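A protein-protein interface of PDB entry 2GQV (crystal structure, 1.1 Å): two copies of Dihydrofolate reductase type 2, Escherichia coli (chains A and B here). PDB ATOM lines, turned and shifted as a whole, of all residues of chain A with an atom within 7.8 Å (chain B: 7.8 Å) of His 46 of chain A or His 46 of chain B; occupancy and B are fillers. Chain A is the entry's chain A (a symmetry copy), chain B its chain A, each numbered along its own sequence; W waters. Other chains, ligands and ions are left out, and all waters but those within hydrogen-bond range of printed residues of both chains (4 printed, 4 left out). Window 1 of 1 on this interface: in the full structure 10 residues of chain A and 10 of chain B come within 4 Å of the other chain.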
ATOM      1  N   VAL A  14      34.356 -27.766  21.727  1.00  0.00           N
ATOM      2  CA  VAL A  14      33.019 -28.365  21.615  1.00  0.00           C
ATOM      3  C   VAL A  14      32.366 -27.902  20.335  1.00  0.00           C
ATOM      4  O   VAL A  14      32.717 -26.919  19.721  1.00  0.00           O
ATOM      5  CB  VAL A  14      32.165 -28.056  22.863  1.00  0.00           C
ATOM      6  CG1 VAL A  14      32.724 -28.570  24.156  1.00  0.00           C
ATOM      7  CG2 VAL A  14      31.883 -26.529  22.944  1.00  0.00           C
ATOM      8  N   ARG A  15      31.340 -28.676  19.950  1.00  0.00           N
ATOM      9  CA  ARG A  15      30.445 -28.310  18.878  1.00  0.00           C
ATOM     10  C   ARG A  15      29.011 -28.608  19.207  1.00  0.00           C
ATOM     11  O   ARG A  15      28.689 -29.487  20.043  1.00  0.00           O
ATOM     12  CB  ARG A  15      30.800 -29.046  17.594  1.00  0.00           C
ATOM     13  CG  ARG A  15      30.632 -30.533  17.609  1.00  0.00           C
ATOM     14  CD  ARG A  15      30.995 -31.162  16.270  1.00  0.00           C
ATOM     15  NE  ARG A  15      30.621 -32.579  16.271  1.00  0.00           N
ATOM     16  CZ  ARG A  15      31.166 -33.424  15.351  1.00  0.00           C
ATOM     17  NH1 ARG A  15      32.092 -33.137  14.414  1.00  0.00           N
ATOM     18  NH2 ARG A  15      30.651 -34.677  15.525  1.00  0.00           N
ATOM     19  N   GLY A  19      21.264 -29.427  14.419  1.00  0.00           N
ATOM     20  CA  GLY A  19      20.656 -28.162  14.084  1.00  0.00           C
ATOM     21  C   GLY A  19      21.649 -27.110  13.781  1.00  0.00           C
ATOM     22  O   GLY A  19      22.664 -27.381  13.111  1.00  0.00           O
ATOM     23  N   ALA A  20      21.426 -25.889  14.231  1.00  0.00           N
ATOM     24  CA  ALA A  20      22.353 -24.794  13.947  1.00  0.00           C
ATOM     25  C   ALA A  20      23.708 -25.137  14.407  1.00  0.00           C
ATOM     26  O   ALA A  20      23.930 -25.647  15.552  1.00  0.00           O
ATOM     27  CB  ALA A  20      21.861 -23.529  14.639  1.00  0.00           C
ATOM     28  N   ALA A  21      24.751 -24.890  13.598  1.00  0.00           N
ATOM     29  CA  ALA A  21      26.095 -25.265  13.936  1.00  0.00           C
ATOM     30  C   ALA A  21      26.770 -24.212  14.803  1.00  0.00           C
ATOM     31  O   ALA A  21      26.523 -23.008  14.735  1.00  0.00           O
ATOM     32  CB  ALA A  21      26.919 -25.455  12.645  1.00  0.00           C
ATOM     33  N   TRP A  22      27.732 -24.684  15.632  1.00  0.00           N
ATOM     34  CA  TRP A  22      28.609 -23.802  16.361  1.00  0.00           C
ATOM     35  C   TRP A  22      29.776 -24.632  16.794  1.00  0.00           C
ATOM     36  O   TRP A  22      29.627 -25.816  17.150  1.00  0.00           O
ATOM     37  CB  TRP A  22      27.902 -23.216  17.602  1.00  0.00           C
ATOM     38  CG  TRP A  22      28.600 -22.043  18.216  1.00  0.00           C
ATOM     39  CD1 TRP A  22      29.385 -21.990  19.291  1.00  0.00           C
ATOM     40  CD2 TRP A  22      28.492 -20.698  17.730  1.00  0.00           C
ATOM     41  NE1 TRP A  22      29.805 -20.683  19.513  1.00  0.00           N
ATOM     42  CE2 TRP A  22      29.256 -19.890  18.590  1.00  0.00           C
ATOM     43  CE3 TRP A  22      27.809 -20.100  16.697  1.00  0.00           C
ATOM     44  CZ2 TRP A  22      29.348 -18.499  18.439  1.00  0.00           C
ATOM     45  CZ3 TRP A  22      27.938 -18.739  16.549  1.00  0.00           C
ATOM     46  CH2 TRP A  22      28.706 -17.985  17.412  1.00  0.00           C
ATOM     47  N   GLN A  23      31.006 -24.079  16.845  1.00  0.00           N
ATOM     48  CA  GLN A  23      32.189 -24.829  17.227  1.00  0.00           C
ATOM     49  C   GLN A  23      33.220 -23.909  17.742  1.00  0.00           C
ATOM     50  O   GLN A  23      33.463 -22.854  17.099  1.00  0.00           O
ATOM     51  CB  GLN A  23      32.661 -25.678  16.048  1.00  0.00           C
ATOM     52  CG  GLN A  23      33.798 -26.625  16.304  1.00  0.00           C
ATOM     53  CD  GLN A  23      33.985 -27.588  15.193  1.00  0.00           C
ATOM     54  OE1 GLN A  23      35.125 -27.554  14.549  1.00  0.00           O
ATOM     55  NE2 GLN A  23      33.069 -28.387  14.935  1.00  0.00           N
ATOM     56  N   GLY A  24      33.822 -24.292  18.839  1.00  0.00           N
ATOM     57  CA  GLY A  24      34.906 -23.476  19.415  1.00  0.00           C
ATOM     58  C   GLY A  24      35.155 -23.830  20.855  1.00  0.00           C
ATOM     59  O   GLY A  24      34.818 -24.953  21.289  1.00  0.00           O
ATOM     60  N   VAL A  41      30.266 -20.548  24.536  1.00  0.00           N
ATOM     61  CA  VAL A  41      31.229 -21.082  23.578  1.00  0.00           C
ATOM     62  C   VAL A  41      31.635 -19.983  22.619  1.00  0.00           C
ATOM     63  O   VAL A  41      30.780 -19.377  21.970  1.00  0.00           O
ATOM     64  CB  VAL A  41      30.629 -22.282  22.793  1.00  0.00           C
ATOM     65  CG1 VAL A  41      31.689 -22.857  21.878  1.00  0.00           C
ATOM     66  CG2 VAL A  41      30.064 -23.346  23.695  1.00  0.00           C
ATOM     67  N   GLU A  42      32.931 -19.668  22.559  1.00  0.00           N
ATOM     68  CA  GLU A  42      33.458 -18.688  21.614  1.00  0.00           C
ATOM     69  C   GLU A  42      33.719 -19.391  20.307  1.00  0.00           C
ATOM     70  O   GLU A  42      34.468 -20.390  20.238  1.00  0.00           O
ATOM     71  CB  GLU A  42      34.726 -18.042  22.141  1.00  0.00           C
ATOM     72  CG  GLU A  42      35.230 -16.903  21.222  1.00  0.00           C
ATOM     73  CD  GLU A  42      36.426 -16.194  21.670  1.00  0.00           C
ATOM     74  OE1 GLU A  42      37.075 -16.639  22.642  1.00  0.00           O
ATOM     75  OE2 GLU A  42      36.800 -15.147  21.058  1.00  0.00           O
ATOM     76  N   SER A  43      33.145 -18.894  19.203  1.00  0.00           N
ATOM     77  CA  SER A  43      33.425 -19.519  17.907  1.00  0.00           C
ATOM     78  C   SER A  43      34.907 -19.475  17.570  1.00  0.00           C
ATOM     79  O   SER A  43      35.558 -18.436  17.714  1.00  0.00           O
ATOM     80  CB  SER A  43      32.671 -18.752  16.836  1.00  0.00           C
ATOM     81  OG  SER A  43      33.045 -19.190  15.532  1.00  0.00           O
ATOM     82  N   GLU A  44      35.394 -20.584  17.023  1.00  0.00           N
ATOM     83  CA  GLU A  44      36.748 -20.658  16.502  1.00  0.00           C
ATOM     84  C   GLU A  44      36.847 -20.039  15.109  1.00  0.00           C
ATOM     85  O   GLU A  44      37.983 -19.762  14.667  1.00  0.00           O
ATOM     86  CB  GLU A  44      37.299 -22.065  16.509  1.00  0.00           C
ATOM     87  CG  GLU A  44      36.658 -23.044  15.664  1.00  0.00           C
ATOM     88  CD  GLU A  44      36.954 -24.501  15.865  1.00  0.00           C
ATOM     89  OE1 GLU A  44      37.230 -24.916  17.017  1.00  0.00           O
ATOM     90  OE2 GLU A  44      36.831 -25.303  14.842  1.00  0.00           O
ATOM     91  N   ALA A  45      35.744 -19.899  14.427  1.00  0.00           N
ATOM     92  CA  ALA A  45      35.693 -19.257  13.120  1.00  0.00           C
ATOM     93  C   ALA A  45      35.521 -17.737  13.187  1.00  0.00           C
ATOM     94  O   ALA A  45      35.988 -17.037  12.289  1.00  0.00           O
ATOM     95  CB  ALA A  45      34.563 -19.837  12.295  1.00  0.00           C
ATOM     96  N   HIS A  46      34.823 -17.259  14.185  1.00  0.00           N
ATOM     97  CA  HIS A  46      34.413 -15.855  14.328  1.00  0.00           C
ATOM     98  C   HIS A  46      34.894 -15.380  15.702  1.00  0.00           C
ATOM     99  O   HIS A  46      34.095 -15.309  16.665  1.00  0.00           O
ATOM    100  CB  HIS A  46      32.914 -15.730  14.217  1.00  0.00           C
ATOM    101  CG  HIS A  46      32.287 -16.217  12.938  1.00  0.00           C
ATOM    102  ND1 HIS A  46      32.698 -15.866  11.715  1.00  0.00           N
ATOM    103  CD2 HIS A  46      31.222 -17.011  12.722  1.00  0.00           C
ATOM    104  CE1 HIS A  46      31.825 -16.431  10.818  1.00  0.00           C
ATOM    105  NE2 HIS A  46      30.927 -17.128  11.419  1.00  0.00           N
ATOM    106  N   PRO A  47      36.145 -15.031  15.839  1.00  0.00           N
ATOM    107  CA  PRO A  47      36.692 -14.613  17.123  1.00  0.00           C
ATOM    108  C   PRO A  47      35.866 -13.487  17.774  1.00  0.00           C
ATOM    109  O   PRO A  47      35.444 -12.549  17.121  1.00  0.00           O
ATOM    110  CB  PRO A  47      38.096 -14.096  16.750  1.00  0.00           C
ATOM    111  CG  PRO A  47      38.495 -14.866  15.556  1.00  0.00           C
ATOM    112  CD  PRO A  47      37.189 -15.027  14.743  1.00  0.00           C
ATOM    113  N   GLY A  48      35.635 -13.606  19.055  1.00  0.00           N
ATOM    114  CA  GLY A  48      34.883 -12.666  19.827  1.00  0.00           C
ATOM    115  C   GLY A  48      33.407 -12.927  19.899  1.00  0.00           C
ATOM    116  O   GLY A  48      32.735 -12.383  20.780  1.00  0.00           O
ATOM    117  N   SER A  49      32.860 -13.729  19.007  1.00  0.00           N
ATOM    118  CA  SER A  49      31.412 -14.049  18.991  1.00  0.00           C
ATOM    119  C   SER A  49      31.222 -15.275  19.912  1.00  0.00           C
ATOM    120  O   SER A  49      31.854 -16.328  19.732  1.00  0.00           O
ATOM    121  CB  SER A  49      30.935 -14.316  17.629  1.00  0.00           C
ATOM    122  OG  SER A  49      30.748 -13.035  16.980  1.00  0.00           O
ATOM    123  N   VAL A  50      30.333 -15.130  20.868  1.00  0.00           N
ATOM    124  CA  VAL A  50      30.011 -16.122  21.891  1.00  0.00           C
ATOM    125  C   VAL A  50      28.538 -16.444  21.853  1.00  0.00           C
ATOM    126  O   VAL A  50      27.724 -15.530  21.731  1.00  0.00           O
ATOM    127  CB  VAL A  50      30.431 -15.609  23.324  1.00  0.00           C
ATOM    128  CG1 VAL A  50      30.093 -16.619  24.396  1.00  0.00           C
ATOM    129  CG2 VAL A  50      31.875 -15.249  23.388  1.00  0.00           C
ATOM    130  N   GLN A  51      28.195 -17.745  21.927  1.00  0.00           N
ATOM    131  CA  GLN A  51      26.821 -18.146  22.083  1.00  0.00           C
ATOM    132  C   GLN A  51      26.732 -19.102  23.238  1.00  0.00           C
ATOM    133  O   GLN A  51      27.689 -19.778  23.618  1.00  0.00           O
ATOM    134  CB  GLN A  51      26.295 -18.815  20.793  1.00  0.00           C
ATOM    135  CG  GLN A  51      26.135 -17.976  19.562  1.00  0.00           C
ATOM    136  CD  GLN A  51      24.683 -17.680  19.136  1.00  0.00           C
ATOM    137  OE1 GLN A  51      24.259 -17.954  18.003  1.00  0.00           O
ATOM    138  NE2 GLN A  51      23.846 -17.070  19.935  1.00  0.00           N
ATOM    139  N   TYR A  53      24.549 -22.277  25.212  1.00  0.00           N
ATOM    140  CA  TYR A  53      23.749 -23.455  24.977  1.00  0.00           C
ATOM    141  C   TYR A  53      23.689 -24.349  26.184  1.00  0.00           C
ATOM    142  O   TYR A  53      24.611 -24.476  26.968  1.00  0.00           O
ATOM    143  CB  TYR A  53      24.337 -24.331  23.838  1.00  0.00           C
ATOM    144  CG  TYR A  53      24.559 -23.567  22.550  1.00  0.00           C
ATOM    145  CD1 TYR A  53      23.534 -23.296  21.640  1.00  0.00           C
ATOM    146  CD2 TYR A  53      25.798 -23.120  22.183  1.00  0.00           C
ATOM    147  CE1 TYR A  53      23.800 -22.594  20.493  1.00  0.00           C
ATOM    148  CE2 TYR A  53      26.073 -22.426  21.018  1.00  0.00           C
ATOM    149  CZ  TYR A  53      25.047 -22.175  20.199  1.00  0.00           C
ATOM    150  OH  TYR A  53      25.378 -21.556  18.992  1.00  0.00           O
ATOM    151  N   VAL B  14      28.349 -10.418   3.714  1.00  0.00           N
ATOM    152  CA  VAL B  14      28.720  -9.325   4.624  1.00  0.00           C
ATOM    153  C   VAL B  14      29.546  -9.876   5.762  1.00  0.00           C
ATOM    154  O   VAL B  14      29.561 -11.046   6.073  1.00  0.00           O
ATOM    155  CB  VAL B  14      27.472  -8.559   5.111  1.00  0.00           C
ATOM    156  CG1 VAL B  14      26.660  -7.916   4.028  1.00  0.00           C
ATOM    157  CG2 VAL B  14      26.591  -9.492   5.991  1.00  0.00           C
ATOM    158  N   ARG B  15      30.251  -8.937   6.412  1.00  0.00           N
ATOM    159  CA  ARG B  15      30.943  -9.200   7.650  1.00  0.00           C
ATOM    160  C   ARG B  15      30.778  -8.085   8.642  1.00  0.00           C
ATOM    161  O   ARG B  15      30.520  -6.909   8.285  1.00  0.00           O
ATOM    162  CB  ARG B  15      32.431  -9.406   7.412  1.00  0.00           C
ATOM    163  CG  ARG B  15      33.196  -8.224   6.904  1.00  0.00           C
ATOM    164  CD  ARG B  15      34.676  -8.537   6.722  1.00  0.00           C
ATOM    165  NE  ARG B  15      35.409  -7.304   6.424  1.00  0.00           N
ATOM    166  CZ  ARG B  15      36.652  -7.373   5.868  1.00  0.00           C
ATOM    167  NH1 ARG B  15      37.324  -8.477   5.484  1.00  0.00           N
ATOM    168  NH2 ARG B  15      37.148  -6.110   5.709  1.00  0.00           N
ATOM    169  N   GLY B  19      35.053  -5.490  16.298  1.00  0.00           N
ATOM    170  CA  GLY B  19      34.654  -6.241  17.464  1.00  0.00           C
ATOM    171  C   GLY B  19      34.387  -7.663  17.168  1.00  0.00           C
ATOM    172  O   GLY B  19      35.128  -8.291  16.387  1.00  0.00           O
ATOM    173  N   ALA B  20      33.356  -8.244  17.754  1.00  0.00           N
ATOM    174  CA  ALA B  20      33.048  -9.655  17.526  1.00  0.00           C
ATOM    175  C   ALA B  20      32.876  -9.918  16.088  1.00  0.00           C
ATOM    176  O   ALA B  20      32.179  -9.164  15.337  1.00  0.00           O
ATOM    177  CB  ALA B  20      31.780 -10.020  18.288  1.00  0.00           C
ATOM    178  N   ALA B  21      33.465 -10.998  15.551  1.00  0.00           N
ATOM    179  CA  ALA B  21      33.414 -11.285  14.145  1.00  0.00           C
ATOM    180  C   ALA B  21      32.143 -12.033  13.770  1.00  0.00           C
ATOM    181  O   ALA B  21      31.560 -12.813  14.523  1.00  0.00           O
ATOM    182  CB  ALA B  21      34.635 -12.140  13.746  1.00  0.00           C
ATOM    183  N   TRP B  22      31.714 -11.833  12.500  1.00  0.00           N
ATOM    184  CA  TRP B  22      30.657 -12.623  11.921  1.00  0.00           C
ATOM    185  C   TRP B  22      30.760 -12.442  10.439  1.00  0.00           C
ATOM    186  O   TRP B  22      31.076 -11.343   9.945  1.00  0.00           O
ATOM    187  CB  TRP B  22      29.273 -12.141  12.407  1.00  0.00           C
ATOM    188  CG  TRP B  22      28.155 -13.099  12.139  1.00  0.00           C
ATOM    189  CD1 TRP B  22      27.236 -13.083  11.174  1.00  0.00           C
ATOM    190  CD2 TRP B  22      27.856 -14.236  12.961  1.00  0.00           C
ATOM    191  NE1 TRP B  22      26.372 -14.163  11.319  1.00  0.00           N
ATOM    192  CE2 TRP B  22      26.723 -14.855  12.405  1.00  0.00           C
ATOM    193  CE3 TRP B  22      28.400 -14.763  14.109  1.00  0.00           C
ATOM    194  CZ2 TRP B  22      26.122 -15.986  12.977  1.00  0.00           C
ATOM    195  CZ3 TRP B  22      27.814 -15.890  14.635  1.00  0.00           C
ATOM    196  CH2 TRP B  22      26.706 -16.470  14.052  1.00  0.00           C
ATOM    197  N   GLN B  23      30.461 -13.471   9.618  1.00  0.00           N
ATOM    198  CA  GLN B  23      30.565 -13.380   8.173  1.00  0.00           C
ATOM    199  C   GLN B  23      29.674 -14.371   7.543  1.00  0.00           C
ATOM    200  O   GLN B  23      29.672 -15.549   7.987  1.00  0.00           O
ATOM    201  CB  GLN B  23      32.028 -13.520   7.755  1.00  0.00           C
ATOM    202  CG  GLN B  23      32.342 -13.314   6.301  1.00  0.00           C
ATOM    203  CD  GLN B  23      33.798 -13.191   6.055  1.00  0.00           C
ATOM    204  OE1 GLN B  23      34.361 -14.095   5.292  1.00  0.00           O
ATOM    205  NE2 GLN B  23      34.410 -12.237   6.562  1.00  0.00           N
ATOM    206  N   GLY B  24      28.960 -13.931   6.538  1.00  0.00           N
ATOM    207  CA  GLY B  24      28.074 -14.847   5.800  1.00  0.00           C
ATOM    208  C   GLY B  24      27.042 -14.094   5.005  1.00  0.00           C
ATOM    209  O   GLY B  24      27.255 -12.907   4.674  1.00  0.00           O
ATOM    210  N   VAL B  41      22.045 -12.321   9.489  1.00  0.00           N
ATOM    211  CA  VAL B  41      23.168 -12.855   8.724  1.00  0.00           C
ATOM    212  C   VAL B  41      23.417 -14.288   9.143  1.00  0.00           C
ATOM    213  O   VAL B  41      23.625 -14.563  10.325  1.00  0.00           O
ATOM    214  CB  VAL B  41      24.449 -12.002   8.946  1.00  0.00           C
ATOM    215  CG1 VAL B  41      25.560 -12.538   8.069  1.00  0.00           C
ATOM    216  CG2 VAL B  41      24.226 -10.535   8.696  1.00  0.00           C
ATOM    217  N   GLU B  42      23.340 -15.226   8.196  1.00  0.00           N
ATOM    218  CA  GLU B  42      23.643 -16.630   8.456  1.00  0.00           C
ATOM    219  C   GLU B  42      25.131 -16.821   8.318  1.00  0.00           C
ATOM    220  O   GLU B  42      25.737 -16.515   7.267  1.00  0.00           O
ATOM    221  CB  GLU B  42      22.892 -17.541   7.501  1.00  0.00           C
ATOM    222  CG  GLU B  42      23.088 -19.038   7.842  1.00  0.00           C
ATOM    223  CD  GLU B  42      22.370 -19.991   7.000  1.00  0.00           C
ATOM    224  OE1 GLU B  42      21.797 -19.584   5.964  1.00  0.00           O
ATOM    225  OE2 GLU B  42      22.350 -21.218   7.319  1.00  0.00           O
ATOM    226  N   SER B  43      25.791 -17.363   9.351  1.00  0.00           N
ATOM    227  CA  SER B  43      27.230 -17.616   9.227  1.00  0.00           C
ATOM    228  C   SER B  43      27.537 -18.574   8.087  1.00  0.00           C
ATOM    229  O   SER B  43      26.886 -19.614   7.943  1.00  0.00           O
ATOM    230  CB  SER B  43      27.715 -18.246  10.521  1.00  0.00           C
ATOM    231  OG  SER B  43      29.064 -18.689  10.401  1.00  0.00           O
ATOM    232  N   GLU B  44      28.599 -18.258   7.355  1.00  0.00           N
ATOM    233  CA  GLU B  44      29.120 -19.142   6.327  1.00  0.00           C
ATOM    234  C   GLU B  44      29.981 -20.252   6.927  1.00  0.00           C
ATOM    235  O   GLU B  44      30.244 -21.245   6.214  1.00  0.00           O
ATOM    236  CB  GLU B  44      29.870 -18.401   5.245  1.00  0.00           C
ATOM    237  CG  GLU B  44      31.085 -17.714   5.617  1.00  0.00           C
ATOM    238  CD  GLU B  44      31.689 -16.718   4.672  1.00  0.00           C
ATOM    239  OE1 GLU B  44      30.936 -16.059   3.913  1.00  0.00           O
ATOM    240  OE2 GLU B  44      32.977 -16.511   4.733  1.00  0.00           O
ATOM    241  N   ALA B  45      30.455 -20.070   8.128  1.00  0.00           N
ATOM    242  CA  ALA B  45      31.227 -21.081   8.841  1.00  0.00           C
ATOM    243  C   ALA B  45      30.365 -22.072   9.627  1.00  0.00           C
ATOM    244  O   ALA B  45      30.774 -23.220   9.802  1.00  0.00           O
ATOM    245  CB  ALA B  45      32.200 -20.420   9.795  1.00  0.00           C
ATOM    246  N   HIS B  46      29.245 -21.621  10.131  1.00  0.00           N
ATOM    247  CA  HIS B  46      28.373 -22.370  11.047  1.00  0.00           C
ATOM    248  C   HIS B  46      26.970 -22.373  10.434  1.00  0.00           C
ATOM    249  O   HIS B  46      26.090 -21.586  10.857  1.00  0.00           O
ATOM    250  CB  HIS B  46      28.358 -21.721  12.408  1.00  0.00           C
ATOM    251  CG  HIS B  46      29.682 -21.590  13.110  1.00  0.00           C
ATOM    252  ND1 HIS B  46      30.549 -22.594  13.278  1.00  0.00           N
ATOM    253  CD2 HIS B  46      30.253 -20.543  13.735  1.00  0.00           C
ATOM    254  CE1 HIS B  46      31.584 -22.112  14.042  1.00  0.00           C
ATOM    255  NE2 HIS B  46      31.413 -20.869  14.323  1.00  0.00           N
ATOM    256  N   PRO B  47      26.706 -23.227   9.482  1.00  0.00           N
ATOM    257  CA  PRO B  47      25.411 -23.262   8.815  1.00  0.00           C
ATOM    258  C   PRO B  47      24.241 -23.368   9.813  1.00  0.00           C
ATOM    259  O   PRO B  47      24.289 -24.115  10.774  1.00  0.00           O
ATOM    260  CB  PRO B  47      25.496 -24.541   7.958  1.00  0.00           C
ATOM    261  CG  PRO B  47      26.928 -24.706   7.640  1.00  0.00           C
ATOM    262  CD  PRO B  47      27.666 -24.255   8.923  1.00  0.00           C
ATOM    263  N   GLY B  48      23.207 -22.603   9.576  1.00  0.00           N
ATOM    264  CA  GLY B  48      22.035 -22.559  10.393  1.00  0.00           C
ATOM    265  C   GLY B  48      22.068 -21.560  11.513  1.00  0.00           C
ATOM    266  O   GLY B  48      21.014 -21.222  12.058  1.00  0.00           O
ATOM    267  N   SER B  49      23.232 -21.073  11.895  1.00  0.00           N
ATOM    268  CA  SER B  49      23.372 -20.085  12.991  1.00  0.00           C
ATOM    269  C   SER B  49      23.228 -18.688  12.346  1.00  0.00           C
ATOM    270  O   SER B  49      23.954 -18.329  11.404  1.00  0.00           O
ATOM    271  CB  SER B  49      24.656 -20.231  13.687  1.00  0.00           C
ATOM    272  OG  SER B  49      24.528 -21.351  14.596  1.00  0.00           O
ATOM    273  N   VAL B  50      22.314 -17.911  12.879  1.00  0.00           N
ATOM    274  CA  VAL B  50      21.956 -16.572  12.417  1.00  0.00           C
ATOM    275  C   VAL B  50      22.116 -15.578  13.541  1.00  0.00           C
ATOM    276  O   VAL B  50      21.715 -15.872  14.666  1.00  0.00           O
ATOM    277  CB  VAL B  50      20.481 -16.546  11.855  1.00  0.00           C
ATOM    278  CG1 VAL B  50      20.092 -15.164  11.385  1.00  0.00           C
ATOM    279  CG2 VAL B  50      20.280 -17.540  10.766  1.00  0.00           C
ATOM    280  N   GLN B  51      22.727 -14.415  13.245  1.00  0.00           N
ATOM    281  CA  GLN B  51      22.765 -13.331  14.192  1.00  0.00           C
ATOM    282  C   GLN B  51      22.285 -12.083  13.508  1.00  0.00           C
ATOM    283  O   GLN B  51      22.345 -11.928  12.287  1.00  0.00           O
ATOM    284  CB  GLN B  51      24.198 -13.126  14.733  1.00  0.00           C
ATOM    285  CG  GLN B  51      24.799 -14.190  15.601  1.00  0.00           C
ATOM    286  CD  GLN B  51      24.962 -13.828  17.090  1.00  0.00           C
ATOM    287  OE1 GLN B  51      26.058 -13.896  17.668  1.00  0.00           O
ATOM    288  NE2 GLN B  51      23.938 -13.485  17.828  1.00  0.00           N
ATOM    289  N   TYR B  53      22.213  -7.756  13.395  1.00  0.00           N
ATOM    290  CA  TYR B  53      23.009  -6.576  13.633  1.00  0.00           C
ATOM    291  C   TYR B  53      22.452  -5.367  12.936  1.00  0.00           C
ATOM    292  O   TYR B  53      21.879  -5.419  11.863  1.00  0.00           O
ATOM    293  CB  TYR B  53      24.456  -6.740  13.092  1.00  0.00           C
ATOM    294  CG  TYR B  53      25.155  -7.975  13.620  1.00  0.00           C
ATOM    295  CD1 TYR B  53      25.755  -8.029  14.880  1.00  0.00           C
ATOM    296  CD2 TYR B  53      25.268  -9.113  12.870  1.00  0.00           C
ATOM    297  CE1 TYR B  53      26.369  -9.180  15.301  1.00  0.00           C
ATOM    298  CE2 TYR B  53      25.901 -10.271  13.285  1.00  0.00           C
ATOM    299  CZ  TYR B  53      26.435 -10.270  14.511  1.00  0.00           C
ATOM    300  OH  TYR B  53      27.145 -11.422  14.859  1.00  0.00           O
HETATM  301  O   HOH W   1      28.444 -11.460  17.265  1.00  0.00           O
HETATM  302  O   HOH W   2      24.028 -26.844  10.660  1.00  0.00           O
HETATM  303  O   HOH W   3      36.968 -10.466  16.192  1.00  0.00           O
HETATM  304  O   HOH W   4      23.390 -21.166  17.153  1.00  0.00           O
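O of Pro 47 of chain A lies within hydrogen-bond range of N of Ala 21 of chain B (3.0 Å). OG of Ser 49 of chain A lies within hydrogen-bond range of O of Ala 21 of chain B, at 2.6 Å. The side-chain hydroxyl of Ser 43 of chain B is in hydrogen-bond range of a ring nitrogen (NE2) of His 46 of chain A (2.6 Å). A ring nitrogen (NE2) of His 46 of chain B lies within hydrogen-bond range of the side-chain hydroxyl (OG) of Ser 43 of chain A (2.6 Å). The backbone carbonyl oxygen (O) of Pro 47 of chain B lies within hydrogen-bond range of the backbone NH (N) of Ala 21 of chain A, 3.0 Å away. The side-chain hydroxyl (OG) of Ser 49 of chain B is in hydrogen-bond range of the backbone carbonyl oxygen (O) of Ala 21 of chain A, 2.6 Å away.
The side-chain hydroxyl (OG) of Ser 43 of chain B lies within hydrogen-bond range of the backbone NH (N) of Ala 45 of chain B (3.0 Å). The side-chain hydroxyl (OG) of Ser 43 of chain B lies within hydrogen-bond range of the backbone NH (N) of His 46 of chain B, 2.9 Å away.
Among the printed residues, pairs that only touch across the chains: Ala 20 of chain A with Pro 47 of chain B (3.8 Å), Ala 20 of chain A with Gly 48 of chain B (3.6 Å), Ala 20 of chain A with Ser 49 of chain B (3.4 Å), Ala 21 of chain A with His 46 of chain B (3.2 Å), Trp 22 of chain A with Trp 22 of chain B (3.4 Å), Trp 22 of chain A with His 46 of chain B (3.8 Å), Gln 23 of chain A with His 46 of chain B (3.5 Å), Ala 45 of chain A with Ala 45 of chain B (3.5 Å), Ala 45 of chain A with His 46 of chain B (3.9 Å), His 46 of chain A with Ala 21 of chain B (3.2 Å), His 46 of chain A with Trp 22 of chain B (3.8 Å), His 46 of chain A with Gln 23 of chain B (3.5 Å), His 46 of chain A with Ala 45 of chain B (3.9 Å), His 46 of chain A with His 46 of chain B (3.8 Å), Pro 47 of chain A with Ala 20 of chain B (3.8 Å), Gly 48 of chain A with Ala 20 of chain B (3.6 Å) and Ser 49 of chain A with Ala 20 of chain B (3.4 Å).
Of chain B, only Ala 45 (3.5 Å) and His 46 (3.9 Å) come within 4 Å of Ala 45 of chain A. Of the printed residues of chain A, Ala 20 of chain B touches Pro 47, Gly 48 and Ser 49. Val 41 of chain B touches none of the printed residues of chain A. Pro 47 of chain B touches just these residues of chain A: Ala 20 (3.8 Å) and Ala 21 (3.0 Å). Val 50 of chain B touches none of the printed residues of chain A. The nearest residue of chain B that does not touch His 46 of chain A is Glu 44 of chain B (4.8 Å).
Printed residues of chain B that touch a printed residue of chain A: Ala 20, Ala 21, Trp 22, Gln 23, Ser 43, Ala 45, His 46, Pro 47, Gly 48 and Ser 49. Hydrophobic or aromatic side chains of chain B that line the printed part of chain A: Ala 20, Ala 21, Trp 22, Ala 45, His 46 and Pro 47. Hydrophobic or aromatic side chains of chain A that line the printed part of chain B: Ala 20, Ala 21, Trp 22, Ala 45, His 46 and Pro 47. Among the printed residues, no Asp or Glu carboxylate lies within 4 Å of a Lys or Arg side-chain nitrogen of the other chain.
Ala 20 of chain A touches Pro 47 of chain B, and with the chains exchanged Pro 47 of chain A touches Ala 20 of chain B. Trp 22 of chain A touches His 46 of chain B, and with the chains exchanged His 46 of chain A touches Trp 22 of chain B.
Water W3 bridges the backbone carbonyl oxygen of Pro 47 of chain A (2.7 Å) and the backbone carbonyl oxygen of Gly 19 of chain B (2.9 Å).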
